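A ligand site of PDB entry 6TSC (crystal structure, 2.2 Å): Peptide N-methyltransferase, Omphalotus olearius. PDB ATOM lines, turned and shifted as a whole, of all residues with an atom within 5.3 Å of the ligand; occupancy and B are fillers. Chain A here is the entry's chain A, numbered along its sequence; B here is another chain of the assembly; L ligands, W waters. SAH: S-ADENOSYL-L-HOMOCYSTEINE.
O of Phe 103 lies close to SD of the ligand, 3.4 Å away.
A nitrogen (N3) of the ligand lies close to the backbone carbonyl oxygen (O) of Val 242, 3.3 Å away.
Ile 18 touches the ligand.
Gly 98 touches the ligand (CA to O, 3.4 Å).
CG2 of Val 104 touches N of the ligand, at 3.6 Å.
Ser 128 touches the ligand.
Phe 170 touches the ligand (CA to O2', 3.3 Å).
O of Tyr 210 touches C2 of the ligand, at 3.6 Å.
CA of Ile 211 touches N1 of the ligand, 3.4 Å away.
Ile 6 of chain B touches the ligand (CD1 to O3', 3.9 Å).
MVA 7 of chain B touches the ligand.
Of the 31 residues printed, 20 come within 4 Å of the ligand.
The nearest printed residue that does not touch the ligand is Val 127 (4.3 Å).
The backbone carbonyl oxygen of Thr 244 is in hydrogen-bond range of the backbone NH of Tyr 210.
The backbone NH (N) of Gly 240 sits at hydrogen-bond distance from the side-chain hydroxyl (OG) of Ser 243, 2.9 Å away.
OG of Ser 128 sits at hydrogen-bond distance from N of Glu 130, 3.1 Å away.
The side-chain hydroxyl (OH) of Tyr 97 sits at hydrogen-bond distance from O of MVA 5 of chain B, at 2.7 Å.
Water W1 lies within hydrogen-bond range of O of Tyr 97 (2.6 Å) and N of the ligand (2.9 Å).
OG1 of Thr 244 is in hydrogen-bond range of N3 of the ligand (2.6 Å).
The backbone carbonyl oxygen of Val 102 lies within hydrogen-bond range of a nitrogen (N) of the ligand.
The backbone carbonyl oxygen (O) of Gly 241 lies within hydrogen-bond range of an oxygen (O3') of the ligand (2.7 Å).
The backbone NH (N) of Ala 129 lies within hydrogen-bond range of an oxygen (OXT) of the ligand, 2.7 Å away.
N of Ala 212 lies within hydrogen-bond range of N1 of the ligand (2.8 Å).
The backbone carbonyl oxygen (O) of Ala 212 is in hydrogen-bond range of a nitrogen (N6) of the ligand.
An oxygen (O) of the ligand sits at hydrogen-bond distance from the backbone NH of His 99, 2.8 Å away.
N of the ligand is in hydrogen-bond range of O of His 99 (3.0 Å).
N of Gln 171 is in hydrogen-bond range of O2' of the ligand (3.0 Å).
OE1 of Gln 171 sits close to SD of the ligand (3.6 Å).
An oxygen (O2') of the ligand is in hydrogen-bond range of the backbone carbonyl oxygen (O) of Ser 243.
The backbone carbonyl oxygen (O) of Tyr 97 sits at hydrogen-bond distance from a nitrogen (N) of the ligand (3.3 Å).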
ATOM      1  N   ILE A  18     -24.665  17.437  -5.744  1.00  0.00           N
ATOM      2  CA  ILE A  18     -25.041  18.844  -5.452  1.00  0.00           C
ATOM      3  C   ILE A  18     -24.341  19.292  -4.179  1.00  0.00           C
ATOM      4  O   ILE A  18     -23.672  20.307  -4.182  1.00  0.00           O
ATOM      5  CB  ILE A  18     -26.559  18.959  -5.368  1.00  0.00           C
ATOM      6  CG1 ILE A  18     -27.190  18.524  -6.676  1.00  0.00           C
ATOM      7  CG2 ILE A  18     -26.975  20.367  -4.966  1.00  0.00           C
ATOM      8  CD1 ILE A  18     -26.807  19.403  -7.874  1.00  0.00           C
ATOM      9  N   ILE A  43     -19.560  24.429  -8.427  1.00  0.00           N
ATOM     10  CA  ILE A  43     -20.063  25.703  -7.839  1.00  0.00           C
ATOM     11  C   ILE A  43     -19.244  26.060  -6.602  1.00  0.00           C
ATOM     12  O   ILE A  43     -18.743  27.162  -6.512  1.00  0.00           O
ATOM     13  CB  ILE A  43     -21.561  25.580  -7.524  1.00  0.00           C
ATOM     14  CG1 ILE A  43     -22.319  25.144  -8.772  1.00  0.00           C
ATOM     15  CG2 ILE A  43     -22.084  26.885  -6.937  1.00  0.00           C
ATOM     16  CD1 ILE A  43     -23.819  25.177  -8.634  1.00  0.00           C
ATOM     17  N   TYR A  97     -20.951  19.461 -11.801  1.00  0.00           N
ATOM     18  CA  TYR A  97     -21.692  19.356 -10.523  1.00  0.00           C
ATOM     19  C   TYR A  97     -23.000  18.617 -10.824  1.00  0.00           C
ATOM     20  O   TYR A  97     -23.528  18.687 -11.956  1.00  0.00           O
ATOM     21  CB  TYR A  97     -21.877  20.697  -9.826  1.00  0.00           C
ATOM     22  CG  TYR A  97     -22.888  21.621 -10.441  1.00  0.00           C
ATOM     23  CD1 TYR A  97     -22.525  22.507 -11.458  1.00  0.00           C
ATOM     24  CD2 TYR A  97     -24.205  21.639  -9.990  1.00  0.00           C
ATOM     25  CE1 TYR A  97     -23.462  23.365 -12.033  1.00  0.00           C
ATOM     26  CE2 TYR A  97     -25.147  22.494 -10.550  1.00  0.00           C
ATOM     27  CZ  TYR A  97     -24.768  23.362 -11.565  1.00  0.00           C
ATOM     28  OH  TYR A  97     -25.687  24.213 -12.104  1.00  0.00           O
ATOM     29  N   GLY A  98     -23.475  17.903  -9.827  1.00  0.00           N
ATOM     30  CA  GLY A  98     -24.719  17.113  -9.902  1.00  0.00           C
ATOM     31  C   GLY A  98     -24.484  15.855 -10.722  1.00  0.00           C
ATOM     32  O   GLY A  98     -23.487  15.159 -10.449  1.00  0.00           O
ATOM     33  N   HIS A  99     -25.387  15.601 -11.658  1.00  0.00           N
ATOM     34  CA  HIS A  99     -25.301  14.549 -12.704  1.00  0.00           C
ATOM     35  C   HIS A  99     -24.755  15.232 -13.949  1.00  0.00           C
ATOM     36  O   HIS A  99     -25.322  16.214 -14.418  1.00  0.00           O
ATOM     37  CB  HIS A  99     -26.687  13.916 -12.876  1.00  0.00           C
ATOM     38  CG  HIS A  99     -26.750  12.806 -13.856  1.00  0.00           C
ATOM     39  ND1 HIS A  99     -26.296  12.922 -15.148  1.00  0.00           N
ATOM     40  CD2 HIS A  99     -27.303  11.571 -13.772  1.00  0.00           C
ATOM     41  CE1 HIS A  99     -26.526  11.811 -15.802  1.00  0.00           C
ATOM     42  NE2 HIS A  99     -27.144  10.956 -14.990  1.00  0.00           N
ATOM     43  N   PRO A 100     -23.624  14.747 -14.511  1.00  0.00           N
ATOM     44  CA  PRO A 100     -22.964  15.452 -15.617  1.00  0.00           C
ATOM     45  C   PRO A 100     -23.780  15.504 -16.906  1.00  0.00           C
ATOM     46  O   PRO A 100     -23.374  16.237 -17.750  1.00  0.00           O
ATOM     47  CB  PRO A 100     -21.670  14.659 -15.835  1.00  0.00           C
ATOM     48  CG  PRO A 100     -21.924  13.292 -15.231  1.00  0.00           C
ATOM     49  CD  PRO A 100     -22.935  13.517 -14.120  1.00  0.00           C
ATOM     50  N   VAL A 102     -27.437  15.890 -16.840  1.00  0.00           N
ATOM     51  CA  VAL A 102     -28.786  16.424 -16.509  1.00  0.00           C
ATOM     52  C   VAL A 102     -28.723  17.963 -16.601  1.00  0.00           C
ATOM     53  O   VAL A 102     -28.004  18.602 -15.797  1.00  0.00           O
ATOM     54  CB  VAL A 102     -29.284  15.894 -15.137  1.00  0.00           C
ATOM     55  CG1 VAL A 102     -30.551  16.578 -14.643  1.00  0.00           C
ATOM     56  CG2 VAL A 102     -29.515  14.378 -15.188  1.00  0.00           C
ATOM     57  N   PHE A 103     -29.407  18.530 -17.589  1.00  0.00           N
ATOM     58  CA  PHE A 103     -29.298  19.966 -17.933  1.00  0.00           C
ATOM     59  C   PHE A 103     -27.807  20.333 -18.067  1.00  0.00           C
ATOM     60  O   PHE A 103     -27.306  21.196 -17.337  1.00  0.00           O
ATOM     61  CB  PHE A 103     -30.044  20.798 -16.892  1.00  0.00           C
ATOM     62  CG  PHE A 103     -31.512  20.519 -16.840  1.00  0.00           C
ATOM     63  CD1 PHE A 103     -31.980  19.297 -16.392  1.00  0.00           C
ATOM     64  CD2 PHE A 103     -32.427  21.478 -17.208  1.00  0.00           C
ATOM     65  CE1 PHE A 103     -33.336  19.023 -16.341  1.00  0.00           C
ATOM     66  CE2 PHE A 103     -33.789  21.204 -17.165  1.00  0.00           C
ATOM     67  CZ  PHE A 103     -34.239  19.981 -16.730  1.00  0.00           C
ATOM     68  N   VAL A 104     -27.116  19.657 -18.974  1.00  0.00           N
ATOM     69  CA  VAL A 104     -25.687  19.917 -19.287  1.00  0.00           C
ATOM     70  C   VAL A 104     -25.458  19.638 -20.766  1.00  0.00           C
ATOM     71  O   VAL A 104     -25.483  18.479 -21.168  1.00  0.00           O
ATOM     72  CB  VAL A 104     -24.724  19.083 -18.455  1.00  0.00           C
ATOM     73  CG1 VAL A 104     -23.282  19.416 -18.806  1.00  0.00           C
ATOM     74  CG2 VAL A 104     -24.952  19.282 -16.972  1.00  0.00           C
ATOM     75  N   VAL A 127     -25.717  12.322  -8.649  1.00  0.00           N
ATOM     76  CA  VAL A 127     -26.906  12.796  -7.904  1.00  0.00           C
ATOM     77  C   VAL A 127     -27.308  14.144  -8.468  1.00  0.00           C
ATOM     78  O   VAL A 127     -26.532  15.090  -8.333  1.00  0.00           O
ATOM     79  CB  VAL A 127     -26.569  12.900  -6.416  1.00  0.00           C
ATOM     80  CG1 VAL A 127     -27.682  13.594  -5.640  1.00  0.00           C
ATOM     81  CG2 VAL A 127     -26.214  11.546  -5.832  1.00  0.00           C
ATOM     82  N   SER A 128     -28.479  14.237  -9.080  1.00  0.00           N
ATOM     83  CA  SER A 128     -28.950  15.507  -9.690  1.00  0.00           C
ATOM     84  C   SER A 128     -29.637  16.365  -8.629  1.00  0.00           C
ATOM     85  O   SER A 128     -29.833  15.897  -7.497  1.00  0.00           O
ATOM     86  CB  SER A 128     -29.868  15.226 -10.841  1.00  0.00           C
ATOM     87  OG  SER A 128     -31.155  14.849 -10.386  1.00  0.00           O
ATOM     88  N   ALA A 129     -29.966  17.601  -8.994  1.00  0.00           N
ATOM     89  CA  ALA A 129     -30.784  18.519  -8.188  1.00  0.00           C
ATOM     90  C   ALA A 129     -32.186  17.929  -8.014  1.00  0.00           C
ATOM     91  O   ALA A 129     -32.757  18.137  -6.965  1.00  0.00           O
ATOM     92  CB  ALA A 129     -30.828  19.876  -8.845  1.00  0.00           C
ATOM     93  N   GLU A 130     -32.700  17.206  -9.009  1.00  0.00           N
ATOM     94  CA  GLU A 130     -34.033  16.542  -8.949  1.00  0.00           C
ATOM     95  C   GLU A 130     -33.932  15.391  -7.946  1.00  0.00           C
ATOM     96  O   GLU A 130     -34.901  15.181  -7.207  1.00  0.00           O
ATOM     97  CB  GLU A 130     -34.479  16.095 -10.343  1.00  0.00           C
ATOM     98  CG  GLU A 130     -35.773  15.300 -10.337  1.00  0.00           C
ATOM     99  CD  GLU A 130     -36.488  15.264 -11.674  1.00  0.00           C
ATOM    100  OE1 GLU A 130     -36.383  14.256 -12.388  1.00  0.00           O
ATOM    101  OE2 GLU A 130     -37.177  16.236 -11.977  1.00  0.00           O
ATOM    102  N   LEU A 169     -39.483  22.105 -12.481  1.00  0.00           N
ATOM    103  CA  LEU A 169     -39.001  23.152 -13.419  1.00  0.00           C
ATOM    104  C   LEU A 169     -37.585  23.598 -12.992  1.00  0.00           C
ATOM    105  O   LEU A 169     -37.417  24.126 -11.852  1.00  0.00           O
ATOM    106  CB  LEU A 169     -39.991  24.313 -13.427  1.00  0.00           C
ATOM    107  CG  LEU A 169     -41.343  24.031 -14.087  1.00  0.00           C
ATOM    108  CD1 LEU A 169     -42.159  25.307 -14.228  1.00  0.00           C
ATOM    109  CD2 LEU A 169     -41.188  23.377 -15.445  1.00  0.00           C
ATOM    110  N   PHE A 170     -36.607  23.295 -13.848  1.00  0.00           N
ATOM    111  CA  PHE A 170     -35.184  23.737 -13.737  1.00  0.00           C
ATOM    112  C   PHE A 170     -35.044  25.117 -14.386  1.00  0.00           C
ATOM    113  O   PHE A 170     -35.844  25.464 -15.296  1.00  0.00           O
ATOM    114  CB  PHE A 170     -34.253  22.724 -14.409  1.00  0.00           C
ATOM    115  CG  PHE A 170     -33.816  21.536 -13.590  1.00  0.00           C
ATOM    116  CD1 PHE A 170     -34.747  20.622 -13.108  1.00  0.00           C
ATOM    117  CD2 PHE A 170     -32.478  21.280 -13.366  1.00  0.00           C
ATOM    118  CE1 PHE A 170     -34.344  19.516 -12.391  1.00  0.00           C
ATOM    119  CE2 PHE A 170     -32.067  20.189 -12.632  1.00  0.00           C
ATOM    120  CZ  PHE A 170     -33.005  19.302 -12.147  1.00  0.00           C
ATOM    121  N   GLN A 171     -34.064  25.905 -13.920  1.00  0.00           N
ATOM    122  CA  GLN A 171     -33.653  27.195 -14.539  1.00  0.00           C
ATOM    123  C   GLN A 171     -34.844  28.165 -14.593  1.00  0.00           C
ATOM    124  O   GLN A 171     -35.069  28.805 -15.625  1.00  0.00           O
ATOM    125  CB  GLN A 171     -33.033  26.906 -15.903  1.00  0.00           C
ATOM    126  CG  GLN A 171     -31.870  25.946 -15.795  1.00  0.00           C
ATOM    127  CD  GLN A 171     -30.989  25.926 -17.014  1.00  0.00           C
ATOM    128  OE1 GLN A 171     -29.867  25.415 -16.967  1.00  0.00           O
ATOM    129  NE2 GLN A 171     -31.492  26.474 -18.109  1.00  0.00           N
ATOM    130  N   VAL A 172     -35.561  28.280 -13.477  1.00  0.00           N
ATOM    131  CA  VAL A 172     -36.663  29.262 -13.291  1.00  0.00           C
ATOM    132  C   VAL A 172     -36.031  30.636 -13.028  1.00  0.00           C
ATOM    133  O   VAL A 172     -36.763  31.660 -13.149  1.00  0.00           O
ATOM    134  CB  VAL A 172     -37.594  28.838 -12.143  1.00  0.00           C
ATOM    135  CG1 VAL A 172     -38.314  27.545 -12.485  1.00  0.00           C
ATOM    136  CG2 VAL A 172     -36.867  28.702 -10.814  1.00  0.00           C
ATOM    137  N   CYS A 174     -33.593  32.071 -14.781  1.00  0.00           N
ATOM    138  CA  CYS A 174     -33.075  32.674 -16.026  1.00  0.00           C
ATOM    139  C   CYS A 174     -33.999  32.448 -17.226  1.00  0.00           C
ATOM    140  O   CYS A 174     -33.479  32.030 -18.276  1.00  0.00           O
ATOM    141  CB  CYS A 174     -31.727  32.100 -16.402  1.00  0.00           C
ATOM    142  SG  CYS A 174     -31.605  30.359 -15.963  1.00  0.00           S
ATOM    143  N   TYR A 210     -37.420  25.475  -4.322  1.00  0.00           N
ATOM    144  CA  TYR A 210     -36.436  24.463  -3.852  1.00  0.00           C
ATOM    145  C   TYR A 210     -35.031  24.926  -4.211  1.00  0.00           C
ATOM    146  O   TYR A 210     -34.753  25.136  -5.405  1.00  0.00           O
ATOM    147  CB  TYR A 210     -36.705  23.064  -4.426  1.00  0.00           C
ATOM    148  CG  TYR A 210     -35.696  22.063  -3.925  1.00  0.00           C
ATOM    149  CD1 TYR A 210     -35.529  21.859  -2.569  1.00  0.00           C
ATOM    150  CD2 TYR A 210     -34.848  21.369  -4.779  1.00  0.00           C
ATOM    151  CE1 TYR A 210     -34.587  20.967  -2.079  1.00  0.00           C
ATOM    152  CE2 TYR A 210     -33.904  20.472  -4.301  1.00  0.00           C
ATOM    153  CZ  TYR A 210     -33.767  20.268  -2.950  1.00  0.00           C
ATOM    154  OH  TYR A 210     -32.862  19.379  -2.435  1.00  0.00           O
ATOM    155  N   ILE A 211     -34.195  25.073  -3.176  1.00  0.00           N
ATOM    156  CA  ILE A 211     -32.716  25.119  -3.282  1.00  0.00           C
ATOM    157  C   ILE A 211     -32.115  24.090  -2.329  1.00  0.00           C
ATOM    158  O   ILE A 211     -32.318  24.204  -1.109  1.00  0.00           O
ATOM    159  CB  ILE A 211     -32.171  26.531  -3.024  1.00  0.00           C
ATOM    160  CG1 ILE A 211     -32.866  27.567  -3.915  1.00  0.00           C
ATOM    161  CG2 ILE A 211     -30.659  26.548  -3.197  1.00  0.00           C
ATOM    162  CD1 ILE A 211     -32.594  29.009  -3.538  1.00  0.00           C
ATOM    163  N   ALA A 212     -31.419  23.094  -2.871  1.00  0.00           N
ATOM    164  CA  ALA A 212     -30.713  22.056  -2.095  1.00  0.00           C
ATOM    165  C   ALA A 212     -29.562  22.769  -1.401  1.00  0.00           C
ATOM    166  O   ALA A 212     -28.942  23.593  -2.044  1.00  0.00           O
ATOM    167  CB  ALA A 212     -30.184  20.943  -2.974  1.00  0.00           C
ATOM    168  N   ALA A 213     -29.354  22.503  -0.129  1.00  0.00           N
ATOM    169  CA  ALA A 213     -28.158  22.952   0.600  1.00  0.00           C
ATOM    170  C   ALA A 213     -26.955  22.581  -0.257  1.00  0.00           C
ATOM    171  O   ALA A 213     -26.869  21.439  -0.697  1.00  0.00           O
ATOM    172  CB  ALA A 213     -28.076  22.311   1.956  1.00  0.00           C
ATOM    173  N   GLY A 240     -33.223  32.440  -8.024  1.00  0.00           N
ATOM    174  CA  GLY A 240     -31.892  32.661  -8.630  1.00  0.00           C
ATOM    175  C   GLY A 240     -31.461  31.509  -9.515  1.00  0.00           C
ATOM    176  O   GLY A 240     -32.288  30.656  -9.838  1.00  0.00           O
ATOM    177  N   GLY A 241     -30.175  31.481  -9.872  1.00  0.00           N
ATOM    178  CA  GLY A 241     -29.602  30.542 -10.852  1.00  0.00           C
ATOM    179  C   GLY A 241     -29.623  29.092 -10.373  1.00  0.00           C
ATOM    180  O   GLY A 241     -29.520  28.207 -11.226  1.00  0.00           O
ATOM    181  N   VAL A 242     -29.690  28.850  -9.065  1.00  0.00           N
ATOM    182  CA  VAL A 242     -29.762  27.472  -8.485  1.00  0.00           C
ATOM    183  C   VAL A 242     -31.156  27.221  -7.883  1.00  0.00           C
ATOM    184  O   VAL A 242     -31.254  26.362  -6.995  1.00  0.00           O
ATOM    185  CB  VAL A 242     -28.643  27.215  -7.468  1.00  0.00           C
ATOM    186  CG1 VAL A 242     -27.278  27.253  -8.146  1.00  0.00           C
ATOM    187  CG2 VAL A 242     -28.693  28.144  -6.269  1.00  0.00           C
ATOM    188  N   SER A 243     -32.187  27.915  -8.361  1.00  0.00           N
ATOM    189  CA  SER A 243     -33.588  27.715  -7.914  1.00  0.00           C
ATOM    190  C   SER A 243     -34.270  26.724  -8.840  1.00  0.00           C
ATOM    191  O   SER A 243     -34.144  26.855 -10.061  1.00  0.00           O
ATOM    192  CB  SER A 243     -34.331  29.004  -7.864  1.00  0.00           C
ATOM    193  OG  SER A 243     -33.794  29.818  -6.843  1.00  0.00           O
ATOM    194  N   THR A 244     -34.966  25.754  -8.246  1.00  0.00           N
ATOM    195  CA  THR A 244     -35.819  24.772  -8.952  1.00  0.00           C
ATOM    196  C   THR A 244     -37.220  24.916  -8.358  1.00  0.00           C
ATOM    197  O   THR A 244     -37.299  25.079  -7.103  1.00  0.00           O
ATOM    198  CB  THR A 244     -35.237  23.356  -8.790  1.00  0.00           C
ATOM    199  OG1 THR A 244     -33.944  23.309  -9.379  1.00  0.00           O
ATOM    200  CG2 THR A 244     -36.106  22.282  -9.420  1.00  0.00           C
ATOM    201  N   MVA B   5     -24.557  28.951 -12.204  1.00  0.00           N
ATOM    202  CN  MVA B   5     -25.490  28.253 -11.326  1.00  0.00           C
ATOM    203  CA  MVA B   5     -23.665  28.122 -13.054  1.00  0.00           C
ATOM    204  CB  MVA B   5     -22.682  27.299 -12.200  1.00  0.00           C
ATOM    205  CG1 MVA B   5     -21.666  26.551 -13.052  1.00  0.00           C
ATOM    206  CG2 MVA B   5     -21.968  28.203 -11.216  1.00  0.00           C
ATOM    207  C   MVA B   5     -24.502  27.255 -13.994  1.00  0.00           C
ATOM    208  O   MVA B   5     -24.633  26.054 -13.795  1.00  0.00           O
ATOM    209  N   ILE B   6     -25.077  27.916 -15.000  1.00  0.00           N
ATOM    210  CA  ILE B   6     -26.048  27.296 -15.880  1.00  0.00           C
ATOM    211  C   ILE B   6     -25.301  26.544 -16.986  1.00  0.00           C
ATOM    212  O   ILE B   6     -24.517  27.146 -17.712  1.00  0.00           O
ATOM    213  CB  ILE B   6     -26.977  28.368 -16.462  1.00  0.00           C
ATOM    214  CG1 ILE B   6     -27.566  29.310 -15.400  1.00  0.00           C
ATOM    215  CG2 ILE B   6     -28.066  27.714 -17.297  1.00  0.00           C
ATOM    216  CD1 ILE B   6     -28.648  28.694 -14.548  1.00  0.00           C
ATOM    217  N   MVA B   7     -25.484  25.222 -17.177  1.00  0.00           N
ATOM    218  CN  MVA B   7     -26.543  24.445 -16.547  1.00  0.00           C
ATOM    219  CA  MVA B   7     -24.621  24.509 -18.160  1.00  0.00           C
ATOM    220  CB  MVA B   7     -23.698  23.431 -17.537  1.00  0.00           C
ATOM    221  CG1 MVA B   7     -22.369  23.357 -18.280  1.00  0.00           C
ATOM    222  CG2 MVA B   7     -23.403  23.633 -16.052  1.00  0.00           C
ATOM    223  C   MVA B   7     -25.455  23.957 -19.314  1.00  0.00           C
ATOM    224  O   MVA B   7     -25.065  23.016 -19.993  1.00  0.00           O
ATOM    225  N   VAL B   8     -26.603  24.586 -19.579  1.00  0.00           N
ATOM    226  CA  VAL B   8     -27.443  24.270 -20.696  1.00  0.00           C
ATOM    227  C   VAL B   8     -28.229  25.534 -21.085  1.00  0.00           C
ATOM    228  O   VAL B   8     -28.515  26.336 -20.214  1.00  0.00           O
ATOM    229  CB  VAL B   8     -28.377  23.098 -20.351  1.00  0.00           C
ATOM    230  CG1 VAL B   8     -29.680  23.570 -19.723  1.00  0.00           C
ATOM    231  CG2 VAL B   8     -28.659  22.212 -21.562  1.00  0.00           C
HETATM  232  N   SAH L   1     -26.360  18.961 -13.713  1.00  0.00           N
HETATM  233  CA  SAH L   1     -27.145  19.657 -12.650  1.00  0.00           C
HETATM  234  CB  SAH L   1     -28.143  20.649 -13.253  1.00  0.00           C
HETATM  235  CG  SAH L   1     -27.460  21.813 -13.996  1.00  0.00           C
HETATM  236  SD  SAH L   1     -28.681  22.937 -14.712  1.00  0.00           S
HETATM  237  C   SAH L   1     -27.912  18.623 -11.812  1.00  0.00           C
HETATM  238  O   SAH L   1     -27.518  17.466 -11.783  1.00  0.00           O
HETATM  239  OXT SAH L   1     -28.917  18.918 -11.166  1.00  0.00           O
HETATM  240  C5' SAH L   1     -28.824  24.243 -13.488  1.00  0.00           C
HETATM  241  C4' SAH L   1     -30.132  24.132 -12.747  1.00  0.00           C
HETATM  242  O4' SAH L   1     -30.058  23.006 -11.836  1.00  0.00           O
HETATM  243  C3' SAH L   1     -30.498  25.305 -11.847  1.00  0.00           C
HETATM  244  O3' SAH L   1     -31.054  26.403 -12.558  1.00  0.00           O
HETATM  245  C2' SAH L   1     -31.543  24.629 -10.956  1.00  0.00           C
HETATM  246  O2' SAH L   1     -32.790  24.550 -11.627  1.00  0.00           O
HETATM  247  C1' SAH L   1     -30.877  23.271 -10.722  1.00  0.00           C
HETATM  248  N9  SAH L   1     -30.063  23.262  -9.507  1.00  0.00           N
HETATM  249  C8  SAH L   1     -28.698  23.355  -9.407  1.00  0.00           C
HETATM  250  N7  SAH L   1     -28.265  23.368  -8.170  1.00  0.00           N
HETATM  251  C5  SAH L   1     -29.413  23.331  -7.407  1.00  0.00           C
HETATM  252  C6  SAH L   1     -29.635  23.350  -6.025  1.00  0.00           C
HETATM  253  N6  SAH L   1     -28.649  23.440  -5.146  1.00  0.00           N
HETATM  254  N1  SAH L   1     -30.907  23.308  -5.588  1.00  0.00           N
HETATM  255  C2  SAH L   1     -31.900  23.248  -6.489  1.00  0.00           C
HETATM  256  N3  SAH L   1     -31.819  23.209  -7.813  1.00  0.00           N
HETATM  257  C4  SAH L   1     -30.537  23.259  -8.220  1.00  0.00           C
HETATM  258  O   HOH W   1     -23.872  20.454 -13.798  1.00  0.00           O
